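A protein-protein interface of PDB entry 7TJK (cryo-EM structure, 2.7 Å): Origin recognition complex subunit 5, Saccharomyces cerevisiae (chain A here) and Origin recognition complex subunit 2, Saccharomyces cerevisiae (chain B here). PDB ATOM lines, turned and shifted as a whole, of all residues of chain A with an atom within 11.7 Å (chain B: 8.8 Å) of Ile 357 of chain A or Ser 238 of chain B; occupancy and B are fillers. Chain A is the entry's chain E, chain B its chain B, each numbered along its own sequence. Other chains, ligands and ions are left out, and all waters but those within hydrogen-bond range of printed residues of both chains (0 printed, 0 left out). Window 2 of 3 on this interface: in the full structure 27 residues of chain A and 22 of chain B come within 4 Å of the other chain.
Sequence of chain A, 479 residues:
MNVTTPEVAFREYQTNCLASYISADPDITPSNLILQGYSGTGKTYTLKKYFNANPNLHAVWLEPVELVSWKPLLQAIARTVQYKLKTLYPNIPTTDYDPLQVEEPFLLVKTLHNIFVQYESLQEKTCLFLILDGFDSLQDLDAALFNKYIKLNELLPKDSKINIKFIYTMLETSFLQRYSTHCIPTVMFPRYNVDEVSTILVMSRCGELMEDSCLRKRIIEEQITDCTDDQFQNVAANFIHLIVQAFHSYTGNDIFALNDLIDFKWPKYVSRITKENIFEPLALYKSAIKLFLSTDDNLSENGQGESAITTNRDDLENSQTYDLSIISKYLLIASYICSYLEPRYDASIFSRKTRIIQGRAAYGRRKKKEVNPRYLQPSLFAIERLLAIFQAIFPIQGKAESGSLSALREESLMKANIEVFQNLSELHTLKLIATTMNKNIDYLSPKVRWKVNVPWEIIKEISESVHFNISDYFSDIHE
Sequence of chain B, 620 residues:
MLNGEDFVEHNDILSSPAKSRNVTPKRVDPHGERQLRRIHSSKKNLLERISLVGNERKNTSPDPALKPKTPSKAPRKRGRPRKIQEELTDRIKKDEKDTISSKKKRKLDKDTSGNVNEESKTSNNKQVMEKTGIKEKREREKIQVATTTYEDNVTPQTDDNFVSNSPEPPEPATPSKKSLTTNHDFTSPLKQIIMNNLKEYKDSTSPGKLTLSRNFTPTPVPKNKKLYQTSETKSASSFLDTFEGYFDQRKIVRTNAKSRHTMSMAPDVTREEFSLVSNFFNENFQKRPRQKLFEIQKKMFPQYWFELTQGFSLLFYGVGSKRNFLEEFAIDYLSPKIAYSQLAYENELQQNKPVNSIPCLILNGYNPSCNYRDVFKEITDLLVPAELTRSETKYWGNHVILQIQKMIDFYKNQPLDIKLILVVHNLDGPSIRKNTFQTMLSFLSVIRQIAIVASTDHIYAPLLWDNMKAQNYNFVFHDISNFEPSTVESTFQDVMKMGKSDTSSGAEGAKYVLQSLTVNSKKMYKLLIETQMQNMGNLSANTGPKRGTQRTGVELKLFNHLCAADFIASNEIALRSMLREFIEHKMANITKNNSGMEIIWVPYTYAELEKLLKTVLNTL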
ATOM      1  N   ALA A 347     -12.145 -15.397  -5.853  1.00  0.00           N
ATOM      2  CA  ALA A 347     -13.499 -15.448  -6.392  1.00  0.00           C
ATOM      3  C   ALA A 347     -13.553 -15.218  -7.897  1.00  0.00           C
ATOM      4  O   ALA A 347     -14.621 -15.399  -8.493  1.00  0.00           O
ATOM      5  CB  ALA A 347     -14.385 -14.426  -5.680  1.00  0.00           C
ATOM      6  N   SER A 351     -14.494 -19.533  -9.427  1.00  0.00           N
ATOM      7  CA  SER A 351     -15.953 -19.507  -9.381  1.00  0.00           C
ATOM      8  C   SER A 351     -16.531 -19.907 -10.735  1.00  0.00           C
ATOM      9  O   SER A 351     -16.258 -19.256 -11.750  1.00  0.00           O
ATOM     10  CB  SER A 351     -16.448 -18.123  -8.970  1.00  0.00           C
ATOM     11  OG  SER A 351     -16.120 -17.849  -7.620  1.00  0.00           O
ATOM     12  N   ARG A 352     -17.323 -20.982 -10.749  1.00  0.00           N
ATOM     13  CA  ARG A 352     -17.925 -21.488 -11.978  1.00  0.00           C
ATOM     14  C   ARG A 352     -19.358 -21.973 -11.762  1.00  0.00           C
ATOM     15  O   ARG A 352     -19.790 -22.932 -12.410  1.00  0.00           O
ATOM     16  CB  ARG A 352     -17.080 -22.615 -12.578  1.00  0.00           C
ATOM     17  CG  ARG A 352     -16.608 -23.650 -11.567  1.00  0.00           C
ATOM     18  CD  ARG A 352     -15.595 -24.596 -12.191  1.00  0.00           C
ATOM     19  NE  ARG A 352     -14.723 -25.208 -11.195  1.00  0.00           N
ATOM     20  CZ  ARG A 352     -14.990 -26.341 -10.559  1.00  0.00           C
ATOM     21  NH1 ARG A 352     -16.107 -27.013 -10.785  1.00  0.00           N
ATOM     22  NH2 ARG A 352     -14.114 -26.810  -9.677  1.00  0.00           N
ATOM     23  N   LYS A 353     -20.104 -21.343 -10.861  1.00  0.00           N
ATOM     24  CA  LYS A 353     -21.440 -21.802 -10.509  1.00  0.00           C
ATOM     25  C   LYS A 353     -22.501 -20.820 -10.991  1.00  0.00           C
ATOM     26  O   LYS A 353     -22.307 -19.601 -10.963  1.00  0.00           O
ATOM     27  CB  LYS A 353     -21.571 -21.998  -8.997  1.00  0.00           C
ATOM     28  CG  LYS A 353     -22.291 -23.272  -8.584  1.00  0.00           C
ATOM     29  CD  LYS A 353     -22.296 -23.427  -7.070  1.00  0.00           C
ATOM     30  CE  LYS A 353     -23.317 -24.458  -6.615  1.00  0.00           C
ATOM     31  NZ  LYS A 353     -23.079 -24.896  -5.212  1.00  0.00           N
ATOM     32  N   THR A 354     -23.626 -21.372 -11.437  1.00  0.00           N
ATOM     33  CA  THR A 354     -24.765 -20.580 -11.878  1.00  0.00           C
ATOM     34  C   THR A 354     -25.435 -19.920 -10.674  1.00  0.00           C
ATOM     35  O   THR A 354     -25.559 -20.517  -9.602  1.00  0.00           O
ATOM     36  CB  THR A 354     -25.755 -21.473 -12.636  1.00  0.00           C
ATOM     37  OG1 THR A 354     -25.055 -22.197 -13.655  1.00  0.00           O
ATOM     38  CG2 THR A 354     -26.856 -20.655 -13.306  1.00  0.00           C
ATOM     39  N   ARG A 355     -25.859 -18.670 -10.857  1.00  0.00           N
ATOM     40  CA  ARG A 355     -26.383 -17.840  -9.782  1.00  0.00           C
ATOM     41  C   ARG A 355     -27.902 -17.771  -9.851  1.00  0.00           C
ATOM     42  O   ARG A 355     -28.477 -17.557 -10.923  1.00  0.00           O
ATOM     43  CB  ARG A 355     -25.805 -16.423  -9.857  1.00  0.00           C
ATOM     44  CG  ARG A 355     -24.318 -16.341  -9.582  1.00  0.00           C
ATOM     45  CD  ARG A 355     -23.819 -14.906  -9.643  1.00  0.00           C
ATOM     46  NE  ARG A 355     -22.374 -14.823  -9.469  1.00  0.00           N
ATOM     47  CZ  ARG A 355     -21.763 -14.708  -8.297  1.00  0.00           C
ATOM     48  NH1 ARG A 355     -22.444 -14.619  -7.169  1.00  0.00           N
ATOM     49  NH2 ARG A 355     -20.433 -14.676  -8.260  1.00  0.00           N
ATOM     50  N   ILE A 356     -28.545 -17.955  -8.702  1.00  0.00           N
ATOM     51  CA  ILE A 356     -29.976 -17.719  -8.555  1.00  0.00           C
ATOM     52  C   ILE A 356     -30.249 -16.353  -7.946  1.00  0.00           C
ATOM     53  O   ILE A 356     -30.941 -15.527  -8.542  1.00  0.00           O
ATOM     54  CB  ILE A 356     -30.617 -18.829  -7.697  1.00  0.00           C
ATOM     55  CG1 ILE A 356     -30.388 -20.202  -8.313  1.00  0.00           C
ATOM     56  CG2 ILE A 356     -32.106 -18.576  -7.523  1.00  0.00           C
ATOM     57  CD1 ILE A 356     -30.755 -21.306  -7.370  1.00  0.00           C
ATOM     58  N   ILE A 357     -29.717 -16.118  -6.751  1.00  0.00           N
ATOM     59  CA  ILE A 357     -29.754 -14.804  -6.125  1.00  0.00           C
ATOM     60  C   ILE A 357     -28.810 -13.890  -6.892  1.00  0.00           C
ATOM     61  O   ILE A 357     -27.698 -14.296  -7.254  1.00  0.00           O
ATOM     62  CB  ILE A 357     -29.367 -14.909  -4.638  1.00  0.00           C
ATOM     63  CG1 ILE A 357     -30.334 -15.839  -3.901  1.00  0.00           C
ATOM     64  CG2 ILE A 357     -29.347 -13.544  -3.965  1.00  0.00           C
ATOM     65  CD1 ILE A 357     -31.793 -15.453  -4.044  1.00  0.00           C
ATOM     66  N   GLN A 358     -29.266 -12.669  -7.179  1.00  0.00           N
ATOM     67  CA  GLN A 358     -28.482 -11.722  -7.963  1.00  0.00           C
ATOM     68  C   GLN A 358     -27.230 -11.292  -7.197  1.00  0.00           C
ATOM     69  O   GLN A 358     -27.283 -11.000  -5.997  1.00  0.00           O
ATOM     70  CB  GLN A 358     -29.350 -10.526  -8.366  1.00  0.00           C
ATOM     71  CG  GLN A 358     -29.900  -9.667  -7.231  1.00  0.00           C
ATOM     72  CD  GLN A 358     -30.803  -8.555  -7.722  1.00  0.00           C
ATOM     73  OE1 GLN A 358     -30.994  -8.380  -8.925  1.00  0.00           O
ATOM     74  NE2 GLN A 358     -31.366  -7.794  -6.790  1.00  0.00           N
ATOM     75  N   GLY A 359     -26.092 -11.338  -7.880  1.00  0.00           N
ATOM     76  CA  GLY A 359     -24.819 -11.007  -7.275  1.00  0.00           C
ATOM     77  C   GLY A 359     -23.726 -10.877  -8.313  1.00  0.00           C
ATOM     78  O   GLY A 359     -23.777 -11.529  -9.360  1.00  0.00           O
ATOM     79  N   ARG A 360     -22.731 -10.044  -8.035  1.00  0.00           N
ATOM     80  CA  ARG A 360     -21.652  -9.802  -8.979  1.00  0.00           C
ATOM     81  C   ARG A 360     -20.380 -10.502  -8.522  1.00  0.00           C
ATOM     82  O   ARG A 360     -19.973 -10.387  -7.363  1.00  0.00           O
ATOM     83  CB  ARG A 360     -21.406  -8.302  -9.135  1.00  0.00           C
ATOM     84  CG  ARG A 360     -22.593  -7.558  -9.721  1.00  0.00           C
ATOM     85  CD  ARG A 360     -22.402  -6.057  -9.656  1.00  0.00           C
ATOM     86  NE  ARG A 360     -21.535  -5.574 -10.722  1.00  0.00           N
ATOM     87  CZ  ARG A 360     -21.520  -4.324 -11.165  1.00  0.00           C
ATOM     88  NH1 ARG A 360     -22.321  -3.401 -10.656  1.00  0.00           N
ATOM     89  NH2 ARG A 360     -20.679  -3.991 -12.138  1.00  0.00           N
ATOM     90  N   ALA A 361     -19.759 -11.231  -9.444  1.00  0.00           N
ATOM     91  CA  ALA A 361     -18.503 -11.903  -9.162  1.00  0.00           C
ATOM     92  C   ALA A 361     -17.368 -10.885  -9.070  1.00  0.00           C
ATOM     93  O   ALA A 361     -17.486  -9.738  -9.511  1.00  0.00           O
ATOM     94  CB  ALA A 361     -18.199 -12.947 -10.234  1.00  0.00           C
ATOM     95  N   ALA A 362     -16.263 -11.317  -8.469  1.00  0.00           N
ATOM     96  CA  ALA A 362     -15.092 -10.464  -8.342  1.00  0.00           C
ATOM     97  C   ALA A 362     -14.444 -10.237  -9.704  1.00  0.00           C
ATOM     98  O   ALA A 362     -14.461 -11.105 -10.581  1.00  0.00           O
ATOM     99  CB  ALA A 362     -14.087 -11.078  -7.369  1.00  0.00           C
ATOM    100  N   ALA B 236     -28.401 -12.241   0.959  1.00  0.00           N
ATOM    101  CA  ALA B 236     -27.119 -11.642   1.313  1.00  0.00           C
ATOM    102  C   ALA B 236     -25.994 -12.215   0.459  1.00  0.00           C
ATOM    103  O   ALA B 236     -24.972 -11.566   0.249  1.00  0.00           O
ATOM    104  CB  ALA B 236     -26.823 -11.854   2.789  1.00  0.00           C
ATOM    105  N   SER B 237     -26.191 -13.436  -0.033  1.00  0.00           N
ATOM    106  CA  SER B 237     -25.190 -14.101  -0.855  1.00  0.00           C
ATOM    107  C   SER B 237     -25.890 -14.970  -1.889  1.00  0.00           C
ATOM    108  O   SER B 237     -27.011 -15.438  -1.679  1.00  0.00           O
ATOM    109  CB  SER B 237     -24.234 -14.945  -0.004  1.00  0.00           C
ATOM    110  OG  SER B 237     -23.584 -15.928  -0.789  1.00  0.00           O
ATOM    111  N   SER B 238     -25.208 -15.181  -3.016  1.00  0.00           N
ATOM    112  CA  SER B 238     -25.761 -16.023  -4.071  1.00  0.00           C
ATOM    113  C   SER B 238     -25.505 -17.499  -3.792  1.00  0.00           C
ATOM    114  O   SER B 238     -26.364 -18.346  -4.057  1.00  0.00           O
ATOM    115  CB  SER B 238     -25.176 -15.623  -5.425  1.00  0.00           C
ATOM    116  OG  SER B 238     -23.760 -15.661  -5.399  1.00  0.00           O
ATOM    117  N   PHE B 239     -24.331 -17.822  -3.261  1.00  0.00           N
ATOM    118  CA  PHE B 239     -23.992 -19.183  -2.877  1.00  0.00           C
ATOM    119  C   PHE B 239     -23.906 -19.290  -1.359  1.00  0.00           C
ATOM    120  O   PHE B 239     -23.579 -18.326  -0.661  1.00  0.00           O
ATOM    121  CB  PHE B 239     -22.666 -19.625  -3.503  1.00  0.00           C
ATOM    122  CG  PHE B 239     -22.443 -19.105  -4.892  1.00  0.00           C
ATOM    123  CD1 PHE B 239     -23.188 -19.589  -5.957  1.00  0.00           C
ATOM    124  CD2 PHE B 239     -21.483 -18.134  -5.133  1.00  0.00           C
ATOM    125  CE1 PHE B 239     -22.980 -19.112  -7.239  1.00  0.00           C
ATOM    126  CE2 PHE B 239     -21.269 -17.654  -6.410  1.00  0.00           C
ATOM    127  CZ  PHE B 239     -22.018 -18.145  -7.465  1.00  0.00           C
ATOM    128  N   LEU B 240     -24.203 -20.485  -0.854  1.00  0.00           N
ATOM    129  CA  LEU B 240     -24.189 -20.731   0.582  1.00  0.00           C
ATOM    130  C   LEU B 240     -23.112 -21.738   0.950  1.00  0.00           C
ATOM    131  O   LEU B 240     -22.311 -21.502   1.860  1.00  0.00           O
ATOM    132  CB  LEU B 240     -25.555 -21.229   1.057  1.00  0.00           C
ATOM    133  CG  LEU B 240     -26.627 -20.166   1.292  1.00  0.00           C
ATOM    134  CD1 LEU B 240     -27.879 -20.797   1.877  1.00  0.00           C
ATOM    135  CD2 LEU B 240     -26.102 -19.063   2.194  1.00  0.00           C
ATOM    136  N   ASP B 241     -23.083 -22.857   0.243  1.00  0.00           N
ATOM    137  CA  ASP B 241     -22.212 -23.974   0.558  1.00  0.00           C
ATOM    138  C   ASP B 241     -21.055 -24.029  -0.433  1.00  0.00           C
ATOM    139  O   ASP B 241     -20.896 -23.144  -1.280  1.00  0.00           O
ATOM    140  CB  ASP B 241     -23.007 -25.280   0.564  1.00  0.00           C
ATOM    141  CG  ASP B 241     -24.341 -25.141   1.263  1.00  0.00           C
ATOM    142  OD1 ASP B 241     -24.353 -24.851   2.476  1.00  0.00           O
ATOM    143  OD2 ASP B 241     -25.383 -25.313   0.601  1.00  0.00           O
ATOM    144  N   GLU B 244     -17.710 -21.992  -3.576  1.00  0.00           N
ATOM    145  CA  GLU B 244     -18.373 -20.799  -4.092  1.00  0.00           C
ATOM    146  C   GLU B 244     -18.964 -19.970  -2.960  1.00  0.00           C
ATOM    147  O   GLU B 244     -18.819 -18.746  -2.941  1.00  0.00           O
ATOM    148  CB  GLU B 244     -19.462 -21.169  -5.100  1.00  0.00           C
ATOM    149  CG  GLU B 244     -18.990 -21.782  -6.416  1.00  0.00           C
ATOM    150  CD  GLU B 244     -18.724 -23.271  -6.342  1.00  0.00           C
ATOM    151  OE1 GLU B 244     -18.956 -23.874  -5.276  1.00  0.00           O
ATOM    152  OE2 GLU B 244     -18.329 -23.850  -7.374  1.00  0.00           O
ATOM    153  N   GLY B 245     -19.613 -20.628  -1.995  1.00  0.00           N
ATOM    154  CA  GLY B 245     -20.148 -19.914  -0.848  1.00  0.00           C
ATOM    155  C   GLY B 245     -19.079 -19.340   0.056  1.00  0.00           C
ATOM    156  O   GLY B 245     -19.267 -18.264   0.634  1.00  0.00           O
ATOM    157  N   PHE B 247     -15.979 -18.305  -0.928  1.00  0.00           N
ATOM    158  CA  PHE B 247     -15.437 -17.113  -1.573  1.00  0.00           C
ATOM    159  C   PHE B 247     -16.479 -16.006  -1.681  1.00  0.00           C
ATOM    160  O   PHE B 247     -16.126 -14.822  -1.660  1.00  0.00           O
ATOM    161  CB  PHE B 247     -14.882 -17.461  -2.954  1.00  0.00           C
ATOM    162  CG  PHE B 247     -13.731 -18.422  -2.920  1.00  0.00           C
ATOM    163  CD1 PHE B 247     -12.774 -18.341  -1.922  1.00  0.00           C
ATOM    164  CD2 PHE B 247     -13.602 -19.402  -3.891  1.00  0.00           C
ATOM    165  CE1 PHE B 247     -11.712 -19.228  -1.887  1.00  0.00           C
ATOM    166  CE2 PHE B 247     -12.542 -20.290  -3.865  1.00  0.00           C
ATOM    167  CZ  PHE B 247     -11.596 -20.202  -2.861  1.00  0.00           C
ATOM    168  N   ASP B 248     -17.759 -16.368  -1.786  1.00  0.00           N
ATOM    169  CA  ASP B 248     -18.826 -15.385  -1.924  1.00  0.00           C
ATOM    170  C   ASP B 248     -19.096 -14.647  -0.621  1.00  0.00           C
ATOM    171  O   ASP B 248     -19.378 -13.446  -0.636  1.00  0.00           O
ATOM    172  CB  ASP B 248     -20.099 -16.077  -2.413  1.00  0.00           C
ATOM    173  CG  ASP B 248     -21.081 -15.114  -3.042  1.00  0.00           C
ATOM    174  OD1 ASP B 248     -20.652 -14.026  -3.480  1.00  0.00           O
ATOM    175  OD2 ASP B 248     -22.284 -15.444  -3.100  1.00  0.00           O
ATOM    176  N   GLN B 249     -19.032 -15.342   0.511  1.00  0.00           N
ATOM    177  CA  GLN B 249     -19.345 -14.697   1.776  1.00  0.00           C
ATOM    178  C   GLN B 249     -18.161 -13.951   2.374  1.00  0.00           C
ATOM    179  O   GLN B 249     -18.320 -13.312   3.420  1.00  0.00           O
ATOM    180  CB  GLN B 249     -19.886 -15.731   2.768  1.00  0.00           C
ATOM    181  CG  GLN B 249     -21.293 -16.202   2.424  1.00  0.00           C
ATOM    182  CD  GLN B 249     -21.831 -17.227   3.399  1.00  0.00           C
ATOM    183  OE1 GLN B 249     -21.120 -17.684   4.292  1.00  0.00           O
ATOM    184  NE2 GLN B 249     -23.097 -17.591   3.236  1.00  0.00           N
ATOM    185  N   LYS B 251     -16.742 -11.107   1.324  1.00  0.00           N
ATOM    186  CA  LYS B 251     -16.688  -9.829   0.637  1.00  0.00           C
ATOM    187  C   LYS B 251     -16.126  -8.773   1.587  1.00  0.00           C
ATOM    188  O   LYS B 251     -15.676  -9.074   2.695  1.00  0.00           O
ATOM    189  CB  LYS B 251     -18.070  -9.447   0.114  1.00  0.00           C
ATOM    190  CG  LYS B 251     -18.535 -10.289  -1.058  1.00  0.00           C
ATOM    191  CD  LYS B 251     -19.887  -9.828  -1.571  1.00  0.00           C
ATOM    192  CE  LYS B 251     -20.469 -10.831  -2.551  1.00  0.00           C
ATOM    193  NZ  LYS B 251     -19.626 -10.974  -3.770  1.00  0.00           N
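NH1 of Arg 355 of chain A lies within hydrogen-bond range of OG of Ser 238 of chain B.
The backbone carbonyl oxygen (O) of Phe 239 of chain B lies within hydrogen-bond range of the side-chain hydroxyl (OG) of Ser 237 of chain B, 2.4 Å away. OD2 of Asp 248 of chain B lies within hydrogen-bond range of OG of Ser 237 of chain B (2.7 Å). OD2 of Asp 248 of chain B lies within hydrogen-bond range of OG of Ser 238 of chain B. The backbone NH (N) of Phe 239 of chain B is in hydrogen-bond range of the side-chain carboxylate (OD2) of Asp 248 of chain B (3.1 Å). The side-chain carboxylate of Asp 248 of chain B lies within salt-bridge range of the side-chain amino group of Lys 251 of chain B (3.2 Å).
Lys 353 of chain A touches Phe 239 of chain B. Lys 353 of chain A touches Glu 244 of chain B. Thr 354 of chain A touches Phe 239 of chain B (O to CE1, 3.8 Å). Arg 355 of chain A touches Phe 239 of chain B. Ile 357 of chain A touches Ser 237 of chain B (CG2 to O, 3.8 Å). Ile 357 of chain A touches Ser 238 of chain B (O to CB, 3.4 Å). Arg 360 of chain A touches Lys 251 of chain B (O to NZ, 3.7 Å).
Ile 357 of chain A touches just these residues of chain B: Ser 237 and Ser 238. Ser 238 of chain B touches two residues of chain A. Of chain A, only Ile 357 (3.8 Å) comes within 4 Å of Ser 237 of chain B. Phe 239 of chain B touches just these residues of chain A: Lys 353 (3.7 Å), Thr 354 (3.8 Å) and Arg 355 (3.3 Å). No residue of chain A comes within 4 Å of Leu 240 of chain B. No residue of chain A comes within 4 Å of Asp 248 of chain B. Of the printed residues of chain A, Glu 244 of chain B touches Lys 353 (3.6 Å). Printed residues of chain A within 4 Å of Lys 251 of chain B: Arg 360 (3.7 Å). Of the printed residues of chain B, Arg 355 of chain A touches Ser 238 (2.4 Å) and Phe 239 (3.3 Å). The nearest residue of chain B that does not touch Ile 357 of chain A is Ala 236 of chain B (5.2 Å). The nearest printed residue of chain B that does not touch Arg 355 of chain A is Asp 248 of chain B (4.1 Å).
Of the 13 printed residues of chain A, 5 touch a printed residue of chain B. Among the printed residues, no Asp or Glu carboxylate lies within 4 Å of a Lys or Arg side-chain nitrogen of the other chain.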
